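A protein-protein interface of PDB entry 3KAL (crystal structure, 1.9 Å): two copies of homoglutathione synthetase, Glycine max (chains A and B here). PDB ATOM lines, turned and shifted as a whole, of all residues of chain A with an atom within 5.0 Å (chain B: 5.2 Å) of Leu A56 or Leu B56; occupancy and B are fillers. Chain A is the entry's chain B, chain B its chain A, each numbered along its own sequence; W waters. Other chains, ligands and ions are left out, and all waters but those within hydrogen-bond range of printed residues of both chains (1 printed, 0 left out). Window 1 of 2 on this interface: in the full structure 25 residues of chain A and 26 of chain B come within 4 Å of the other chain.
The backbone carbonyl oxygen of Leu A73 is in hydrogen-bond range of the backbone NH of Leu B73 (3.0 Å).
The backbone NH (N) of Gly B70 is in hydrogen-bond range of the side-chain hydroxyl (OG1) of Thr A51 (3.3 Å).
SG of Cys B54 lies within hydrogen-bond range of O of Thr A51 (3.4 Å).
N of His B75 lies within hydrogen-bond range of O of Gly A70, at 2.9 Å.
O of Thr B51 is in hydrogen-bond range of SG of Cys A54 (3.4 Å).
O of Gly B70 lies within hydrogen-bond range of N of His A75 (3.0 Å).
The side-chain hydroxyl of Thr B51 lies close to the backbone NH of Gly A70, 3.4 Å away.
N of Val A57 is in hydrogen-bond range of O of Val A74, 2.8 Å away.
OH of Tyr B245 sits at hydrogen-bond distance from N of Gly B70.
The side-chain hydroxyl of Tyr A245 lies within hydrogen-bond range of the backbone NH of Gly A70 (3.1 Å).
The backbone NH (N) of Val B57 is in hydrogen-bond range of the backbone carbonyl oxygen (O) of Val B74 (2.9 Å).
Among the printed residues, pairs that only touch across the chains: Leu A73 with Leu B56, Leu A56 with Leu B56, Thr A51 with Tyr B245, Tyr A245 with Thr B51, Leu A56 with Leu B73, Gly A70 with Val B74, Val A74 with Gly B70, Leu A73 with Thr B51 and Thr A51 with Leu B73.
Leu A56 touches just these residues of chain B: Leu B56 and Leu B73.
Of chain A, only Leu A56 and Leu A73 come within 4 Å of Leu B56.
Printed residues of chain A within 4 Å of Thr B51: Cys A54 (3.4 Å), Gly A70 (3.3 Å), Leu A73 (3.7 Å) and Tyr A245 (3.5 Å).
Of the printed residues of chain B, Gly A70 touches Thr B51 (3.3 Å), Val B74 (3.5 Å) and His B75 (2.9 Å).
Leu B76 touches none of the printed residues of chain A.
Ser B50 touches none of the printed residues of chain A.
The nearest printed residue of chain A that does not touch Cys B54 is Cys A54 (5.8 Å).
Of the 14 printed residues of chain B, 8 touch a printed residue of chain A.
Hydrophobic or aromatic side chains of chain B within 4 Å of the printed part of chain A: Leu B56, Leu B73, Val B74, His B75 and Tyr B245.
Of the 13 printed residues of chain A, 8 touch a printed residue of chain B.
Printed residues of chain A that touch a printed residue of chain B: Thr A51, Cys A54, Leu A56, Gly A70, Leu A73, Val A74, His A75 and Tyr A245.
Hydrophobic or aromatic side chains of chain A that line the printed part of chain B: Leu A56, Leu A73, Val A74, His A75 and Tyr A245.
Among the printed residues, no Asp or Glu carboxylate lies within 4 Å of a Lys or Arg side-chain nitrogen of the other chain.
Thr A51 touches Cys B54, and with the chains exchanged Cys A54 touches Thr B51.
Thr A51 touches Gly B70, and with the chains exchanged Gly A70 touches Thr B51.
Leu A56 touches its own counterpart, Leu B56.
Gly A70 touches Val B74, and with the chains exchanged Val A74 touches Gly B70.
Positions printed for both chains: 50, 51, 54, 55, 56, 57, 58, 70, 73, 74, 75, 76 and 245.
Water W1 lies within hydrogen-bond range of the backbone carbonyl oxygen (O) of Thr B51, the backbone carbonyl oxygen (O) of Thr A51, the backbone NH (N) of Cys A54 and the backbone NH (N) of Cys B54.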
ATOM      1  N   SER A  50      -4.256 -11.744 -12.081  1.00  0.00           N
ATOM      2  CA  SER A  50      -4.280 -12.780 -11.115  1.00  0.00           C
ATOM      3  C   SER A  50      -3.587 -14.079 -11.735  1.00  0.00           C
ATOM      4  O   SER A  50      -2.809 -14.816 -11.060  1.00  0.00           O
ATOM      5  CB  SER A  50      -5.679 -13.090 -10.516  1.00  0.00           C
ATOM      6  OG  SER A  50      -6.091 -11.989  -9.880  1.00  0.00           O
ATOM      7  N   THR A  51      -3.931 -14.317 -12.985  1.00  0.00           N
ATOM      8  CA  THR A  51      -3.535 -15.562 -13.704  1.00  0.00           C
ATOM      9  C   THR A  51      -2.036 -15.429 -14.034  1.00  0.00           C
ATOM     10  O   THR A  51      -1.258 -16.324 -13.696  1.00  0.00           O
ATOM     11  CB  THR A  51      -4.319 -15.833 -14.973  1.00  0.00           C
ATOM     12  OG1 THR A  51      -5.735 -15.821 -14.621  1.00  0.00           O
ATOM     13  CG2 THR A  51      -3.795 -17.206 -15.579  1.00  0.00           C
ATOM     14  N   CYS A  54       0.191 -15.662 -10.803  1.00  0.00           N
ATOM     15  CA  CYS A  54      -0.144 -16.866  -9.883  1.00  0.00           C
ATOM     16  C   CYS A  54      -0.853 -16.419  -8.559  1.00  0.00           C
ATOM     17  O   CYS A  54      -0.558 -16.973  -7.479  1.00  0.00           O
ATOM     18  CB  CYS A  54       1.203 -17.675  -9.544  1.00  0.00           C
ATOM     19  SG  CYS A  54       0.855 -19.278  -8.951  1.00  0.00           S
ATOM     20  N   LEU A  55      -1.836 -15.451  -8.615  1.00  0.00           N
ATOM     21  CA  LEU A  55      -2.775 -15.306  -7.616  1.00  0.00           C
ATOM     22  C   LEU A  55      -3.853 -16.359  -7.670  1.00  0.00           C
ATOM     23  O   LEU A  55      -4.993 -16.049  -7.961  1.00  0.00           O
ATOM     24  CB  LEU A  55      -3.291 -13.821  -7.473  1.00  0.00           C
ATOM     25  CG  LEU A  55      -4.266 -13.525  -6.341  1.00  0.00           C
ATOM     26  CD1 LEU A  55      -3.505 -13.520  -5.035  1.00  0.00           C
ATOM     27  CD2 LEU A  55      -4.696 -11.992  -6.749  1.00  0.00           C
ATOM     28  N   LEU A  56      -3.455 -17.621  -7.512  1.00  0.00           N
ATOM     29  CA  LEU A  56      -4.236 -18.779  -7.808  1.00  0.00           C
ATOM     30  C   LEU A  56      -4.235 -19.791  -6.702  1.00  0.00           C
ATOM     31  O   LEU A  56      -3.263 -19.909  -5.935  1.00  0.00           O
ATOM     32  CB  LEU A  56      -3.718 -19.455  -9.115  1.00  0.00           C
ATOM     33  CG  LEU A  56      -3.497 -18.641 -10.378  1.00  0.00           C
ATOM     34  CD1 LEU A  56      -2.892 -19.547 -11.530  1.00  0.00           C
ATOM     35  CD2 LEU A  56      -4.972 -18.348 -10.858  1.00  0.00           C
ATOM     36  N   VAL A  57      -5.338 -20.562  -6.528  1.00  0.00           N
ATOM     37  CA  VAL A  57      -5.329 -21.696  -5.618  1.00  0.00           C
ATOM     38  C   VAL A  57      -6.003 -22.834  -6.335  1.00  0.00           C
ATOM     39  O   VAL A  57      -6.610 -22.616  -7.362  1.00  0.00           O
ATOM     40  CB  VAL A  57      -6.178 -21.350  -4.283  1.00  0.00           C
ATOM     41  CG1 VAL A  57      -5.366 -20.386  -3.364  1.00  0.00           C
ATOM     42  CG2 VAL A  57      -7.661 -20.584  -4.689  1.00  0.00           C
ATOM     43  N   GLY A  58      -5.966 -24.058  -5.745  1.00  0.00           N
ATOM     44  CA  GLY A  58      -6.734 -25.166  -6.196  1.00  0.00           C
ATOM     45  C   GLY A  58      -8.232 -24.791  -6.092  1.00  0.00           C
ATOM     46  O   GLY A  58      -8.597 -24.300  -5.060  1.00  0.00           O
ATOM     47  N   GLY A  70      -1.308 -27.830 -10.828  1.00  0.00           N
ATOM     48  CA  GLY A  70      -1.351 -27.624 -12.254  1.00  0.00           C
ATOM     49  C   GLY A  70      -2.678 -27.802 -12.781  1.00  0.00           C
ATOM     50  O   GLY A  70      -2.850 -27.775 -14.020  1.00  0.00           O
ATOM     51  N   LEU A  73      -7.170 -24.979 -11.457  1.00  0.00           N
ATOM     52  CA  LEU A  73      -6.817 -23.723 -10.883  1.00  0.00           C
ATOM     53  C   LEU A  73      -7.930 -22.595 -11.103  1.00  0.00           C
ATOM     54  O   LEU A  73      -8.648 -22.578 -12.133  1.00  0.00           O
ATOM     55  CB  LEU A  73      -5.437 -23.181 -11.403  1.00  0.00           C
ATOM     56  CG  LEU A  73      -4.273 -24.151 -11.280  1.00  0.00           C
ATOM     57  CD1 LEU A  73      -3.280 -23.952 -12.412  1.00  0.00           C
ATOM     58  CD2 LEU A  73      -3.762 -23.856  -9.827  1.00  0.00           C
ATOM     59  N   VAL A  74      -7.955 -21.760 -10.095  1.00  0.00           N
ATOM     60  CA  VAL A  74      -8.872 -20.563  -9.965  1.00  0.00           C
ATOM     61  C   VAL A  74      -8.254 -19.390  -9.195  1.00  0.00           C
ATOM     62  O   VAL A  74      -7.380 -19.616  -8.246  1.00  0.00           O
ATOM     63  CB  VAL A  74     -10.176 -20.996  -9.340  1.00  0.00           C
ATOM     64  CG1 VAL A  74     -10.049 -21.392  -7.858  1.00  0.00           C
ATOM     65  CG2 VAL A  74     -11.358 -19.788  -9.650  1.00  0.00           C
ATOM     66  N   HIS A  75      -8.564 -18.132  -9.613  1.00  0.00           N
ATOM     67  CA  HIS A  75      -7.969 -16.970  -8.902  1.00  0.00           C
ATOM     68  C   HIS A  75      -8.573 -17.011  -7.443  1.00  0.00           C
ATOM     69  O   HIS A  75      -9.749 -17.525  -7.116  1.00  0.00           O
ATOM     70  CB  HIS A  75      -8.327 -15.625  -9.639  1.00  0.00           C
ATOM     71  CG  HIS A  75      -9.813 -15.221  -9.403  1.00  0.00           C
ATOM     72  ND1 HIS A  75     -10.858 -15.683 -10.201  1.00  0.00           N
ATOM     73  CD2 HIS A  75     -10.402 -14.541  -8.385  1.00  0.00           C
ATOM     74  CE1 HIS A  75     -12.010 -15.215  -9.741  1.00  0.00           C
ATOM     75  NE2 HIS A  75     -11.760 -14.606  -8.591  1.00  0.00           N
ATOM     76  N   LEU A  76      -7.821 -16.418  -6.585  1.00  0.00           N
ATOM     77  CA  LEU A  76      -8.113 -16.225  -5.149  1.00  0.00           C
ATOM     78  C   LEU A  76      -9.458 -15.393  -5.109  1.00  0.00           C
ATOM     79  O   LEU A  76      -9.567 -14.395  -5.860  1.00  0.00           O
ATOM     80  CB  LEU A  76      -7.041 -15.417  -4.417  1.00  0.00           C
ATOM     81  CG  LEU A  76      -6.019 -16.028  -3.514  1.00  0.00           C
ATOM     82  CD1 LEU A  76      -6.689 -16.896  -2.395  1.00  0.00           C
ATOM     83  CD2 LEU A  76      -5.087 -17.002  -4.580  1.00  0.00           C
ATOM     84  N   TYR A 245       0.445 -23.309  -3.623  1.00  0.00           N
ATOM     85  CA  TYR A 245       1.319 -22.442  -4.449  1.00  0.00           C
ATOM     86  C   TYR A 245       2.118 -21.435  -3.672  1.00  0.00           C
ATOM     87  O   TYR A 245       3.296 -21.205  -3.924  1.00  0.00           O
ATOM     88  CB  TYR A 245       0.548 -21.796  -5.654  1.00  0.00           C
ATOM     89  CG  TYR A 245      -0.066 -22.962  -6.382  1.00  0.00           C
ATOM     90  CD1 TYR A 245      -1.492 -23.242  -6.241  1.00  0.00           C
ATOM     91  CD2 TYR A 245       0.817 -23.969  -7.127  1.00  0.00           C
ATOM     92  CE1 TYR A 245      -2.090 -24.378  -6.897  1.00  0.00           C
ATOM     93  CE2 TYR A 245       0.206 -25.096  -7.717  1.00  0.00           C
ATOM     94  CZ  TYR A 245      -1.206 -25.239  -7.559  1.00  0.00           C
ATOM     95  OH  TYR A 245      -1.733 -26.262  -8.145  1.00  0.00           O
ATOM     96  N   SER B  50       4.998 -24.988 -13.656  1.00  0.00           N
ATOM     97  CA  SER B  50       4.043 -24.602 -14.691  1.00  0.00           C
ATOM     98  C   SER B  50       3.022 -23.553 -14.030  1.00  0.00           C
ATOM     99  O   SER B  50       2.664 -22.566 -14.659  1.00  0.00           O
ATOM    100  CB  SER B  50       3.327 -25.805 -15.352  1.00  0.00           C
ATOM    101  OG  SER B  50       4.237 -26.566 -15.978  1.00  0.00           O
ATOM    102  N   THR B  51       2.624 -23.824 -12.794  1.00  0.00           N
ATOM    103  CA  THR B  51       1.603 -22.999 -12.056  1.00  0.00           C
ATOM    104  C   THR B  51       2.213 -21.632 -11.666  1.00  0.00           C
ATOM    105  O   THR B  51       1.640 -20.596 -12.000  1.00  0.00           O
ATOM    106  CB  THR B  51       0.924 -23.714 -10.895  1.00  0.00           C
ATOM    107  OG1 THR B  51       0.456 -25.017 -11.320  1.00  0.00           O
ATOM    108  CG2 THR B  51      -0.292 -22.778 -10.286  1.00  0.00           C
ATOM    109  N   CYS B  54       2.959 -19.458 -14.913  1.00  0.00           N
ATOM    110  CA  CYS B  54       1.754 -19.210 -15.804  1.00  0.00           C
ATOM    111  C   CYS B  54       2.030 -19.954 -17.099  1.00  0.00           C
ATOM    112  O   CYS B  54       1.737 -19.454 -18.210  1.00  0.00           O
ATOM    113  CB  CYS B  54       1.550 -17.660 -16.067  1.00  0.00           C
ATOM    114  SG  CYS B  54      -0.045 -17.401 -16.683  1.00  0.00           S
ATOM    115  N   LEU B  55       2.608 -21.212 -16.986  1.00  0.00           N
ATOM    116  CA  LEU B  55       2.485 -22.120 -18.064  1.00  0.00           C
ATOM    117  C   LEU B  55       1.094 -22.751 -18.165  1.00  0.00           C
ATOM    118  O   LEU B  55       0.993 -23.959 -17.969  1.00  0.00           O
ATOM    119  CB  LEU B  55       3.700 -23.105 -18.196  1.00  0.00           C
ATOM    120  CG  LEU B  55       3.766 -24.127 -19.357  1.00  0.00           C
ATOM    121  CD1 LEU B  55       4.070 -23.380 -20.595  1.00  0.00           C
ATOM    122  CD2 LEU B  55       5.052 -25.126 -19.052  1.00  0.00           C
ATOM    123  N   LEU B  56       0.033 -21.957 -18.445  1.00  0.00           N
ATOM    124  CA  LEU B  56      -1.334 -22.306 -18.140  1.00  0.00           C
ATOM    125  C   LEU B  56      -2.226 -21.905 -19.271  1.00  0.00           C
ATOM    126  O   LEU B  56      -1.874 -20.966 -19.999  1.00  0.00           O
ATOM    127  CB  LEU B  56      -1.795 -21.647 -16.849  1.00  0.00           C
ATOM    128  CG  LEU B  56      -1.078 -21.836 -15.514  1.00  0.00           C
ATOM    129  CD1 LEU B  56      -1.698 -20.891 -14.452  1.00  0.00           C
ATOM    130  CD2 LEU B  56      -1.446 -23.322 -15.159  1.00  0.00           C
ATOM    131  N   VAL B  57      -3.320 -22.612 -19.585  1.00  0.00           N
ATOM    132  CA  VAL B  57      -4.266 -22.185 -20.604  1.00  0.00           C
ATOM    133  C   VAL B  57      -5.603 -22.397 -19.981  1.00  0.00           C
ATOM    134  O   VAL B  57      -5.657 -23.048 -18.961  1.00  0.00           O
ATOM    135  CB  VAL B  57      -4.105 -23.035 -21.996  1.00  0.00           C
ATOM    136  CG1 VAL B  57      -2.833 -22.480 -22.764  1.00  0.00           C
ATOM    137  CG2 VAL B  57      -3.884 -24.661 -21.731  1.00  0.00           C
ATOM    138  N   GLY B  58      -6.726 -21.889 -20.561  1.00  0.00           N
ATOM    139  CA  GLY B  58      -8.056 -22.283 -20.134  1.00  0.00           C
ATOM    140  C   GLY B  58      -8.239 -23.791 -20.414  1.00  0.00           C
ATOM    141  O   GLY B  58      -7.769 -24.233 -21.417  1.00  0.00           O
ATOM    142  N   GLY B  70      -8.828 -16.354 -15.535  1.00  0.00           N
ATOM    143  CA  GLY B  70      -8.869 -16.622 -14.108  1.00  0.00           C
ATOM    144  C   GLY B  70      -9.544 -17.843 -13.624  1.00  0.00           C
ATOM    145  O   GLY B  70      -9.642 -18.065 -12.380  1.00  0.00           O
ATOM    146  N   LEU B  73      -8.305 -22.966 -15.084  1.00  0.00           N
ATOM    147  CA  LEU B  73      -6.956 -23.049 -15.560  1.00  0.00           C
ATOM    148  C   LEU B  73      -6.330 -24.493 -15.423  1.00  0.00           C
ATOM    149  O   LEU B  73      -6.703 -25.268 -14.502  1.00  0.00           O
ATOM    150  CB  LEU B  73      -6.047 -22.000 -14.890  1.00  0.00           C
ATOM    151  CG  LEU B  73      -6.549 -20.565 -15.022  1.00  0.00           C
ATOM    152  CD1 LEU B  73      -6.035 -19.779 -13.894  1.00  0.00           C
ATOM    153  CD2 LEU B  73      -6.069 -20.056 -16.355  1.00  0.00           C
ATOM    154  N   VAL B  74      -5.506 -24.771 -16.381  1.00  0.00           N
ATOM    155  CA  VAL B  74      -4.725 -26.054 -16.478  1.00  0.00           C
ATOM    156  C   VAL B  74      -3.334 -25.886 -17.108  1.00  0.00           C
ATOM    157  O   VAL B  74      -3.180 -24.983 -18.002  1.00  0.00           O
ATOM    158  CB  VAL B  74      -5.598 -27.100 -17.176  1.00  0.00           C
ATOM    159  CG1 VAL B  74      -5.735 -26.803 -18.712  1.00  0.00           C
ATOM    160  CG2 VAL B  74      -4.927 -28.631 -16.812  1.00  0.00           C
ATOM    161  N   HIS B  75      -2.298 -26.627 -16.667  1.00  0.00           N
ATOM    162  CA  HIS B  75      -1.028 -26.456 -17.268  1.00  0.00           C
ATOM    163  C   HIS B  75      -1.129 -26.913 -18.744  1.00  0.00           C
ATOM    164  O   HIS B  75      -1.988 -27.794 -19.188  1.00  0.00           O
ATOM    165  CB  HIS B  75       0.045 -27.322 -16.501  1.00  0.00           C
ATOM    166  CG  HIS B  75      -0.162 -28.828 -16.752  1.00  0.00           C
ATOM    167  ND1 HIS B  75       0.390 -29.489 -17.830  1.00  0.00           N
ATOM    168  CD2 HIS B  75      -0.922 -29.761 -16.078  1.00  0.00           C
ATOM    169  CE1 HIS B  75      -0.060 -30.736 -17.838  1.00  0.00           C
ATOM    170  NE2 HIS B  75      -0.768 -30.946 -16.739  1.00  0.00           N
ATOM    171  N   LEU B  76      -0.263 -26.379 -19.530  1.00  0.00           N
ATOM    172  CA  LEU B  76      -0.067 -26.710 -20.965  1.00  0.00           C
ATOM    173  C   LEU B  76       0.264 -28.218 -21.046  1.00  0.00           C
ATOM    174  O   LEU B  76       1.047 -28.729 -20.208  1.00  0.00           O
ATOM    175  CB  LEU B  76       1.074 -25.946 -21.586  1.00  0.00           C
ATOM    176  CG  LEU B  76       0.930 -24.757 -22.421  1.00  0.00           C
ATOM    177  CD1 LEU B  76      -0.008 -24.967 -23.644  1.00  0.00           C
ATOM    178  CD2 LEU B  76       0.188 -23.628 -21.327  1.00  0.00           C
ATOM    179  N   ARG B 242      -8.515 -19.817 -25.447  1.00  0.00           N
ATOM    180  CA  ARG B 242      -7.961 -20.443 -24.230  1.00  0.00           C
ATOM    181  C   ARG B 242      -6.467 -20.161 -24.015  1.00  0.00           C
ATOM    182  O   ARG B 242      -5.947 -20.319 -22.904  1.00  0.00           O
ATOM    183  CB  ARG B 242      -8.229 -22.007 -24.300  1.00  0.00           C
ATOM    184  CG  ARG B 242      -9.660 -22.270 -24.060  1.00  0.00           C
ATOM    185  CD  ARG B 242      -9.977 -23.833 -23.962  1.00  0.00           C
ATOM    186  NE  ARG B 242      -9.398 -24.665 -25.055  1.00  0.00           N
ATOM    187  CZ  ARG B 242      -8.268 -25.454 -24.986  1.00  0.00           C
ATOM    188  NH1 ARG B 242      -7.904 -26.117 -26.080  1.00  0.00           N
ATOM    189  NH2 ARG B 242      -7.455 -25.617 -23.861  1.00  0.00           N
ATOM    190  N   TYR B 245      -3.540 -16.059 -22.246  1.00  0.00           N
ATOM    191  CA  TYR B 245      -2.488 -15.600 -21.341  1.00  0.00           C
ATOM    192  C   TYR B 245      -1.204 -15.184 -21.976  1.00  0.00           C
ATOM    193  O   TYR B 245      -0.606 -14.196 -21.604  1.00  0.00           O
ATOM    194  CB  TYR B 245      -2.314 -16.535 -20.128  1.00  0.00           C
ATOM    195  CG  TYR B 245      -3.670 -16.784 -19.521  1.00  0.00           C
ATOM    196  CD1 TYR B 245      -4.402 -18.014 -19.790  1.00  0.00           C
ATOM    197  CD2 TYR B 245      -4.365 -15.707 -18.739  1.00  0.00           C
ATOM    198  CE1 TYR B 245      -5.741 -18.274 -19.181  1.00  0.00           C
ATOM    199  CE2 TYR B 245      -5.638 -15.940 -18.255  1.00  0.00           C
ATOM    200  CZ  TYR B 245      -6.331 -17.142 -18.539  1.00  0.00           C
ATOM    201  OH  TYR B 245      -7.503 -17.254 -17.973  1.00  0.00           O
HETATM  202  O   HOH W   1       0.648 -18.182 -12.840  1.00  0.00           O
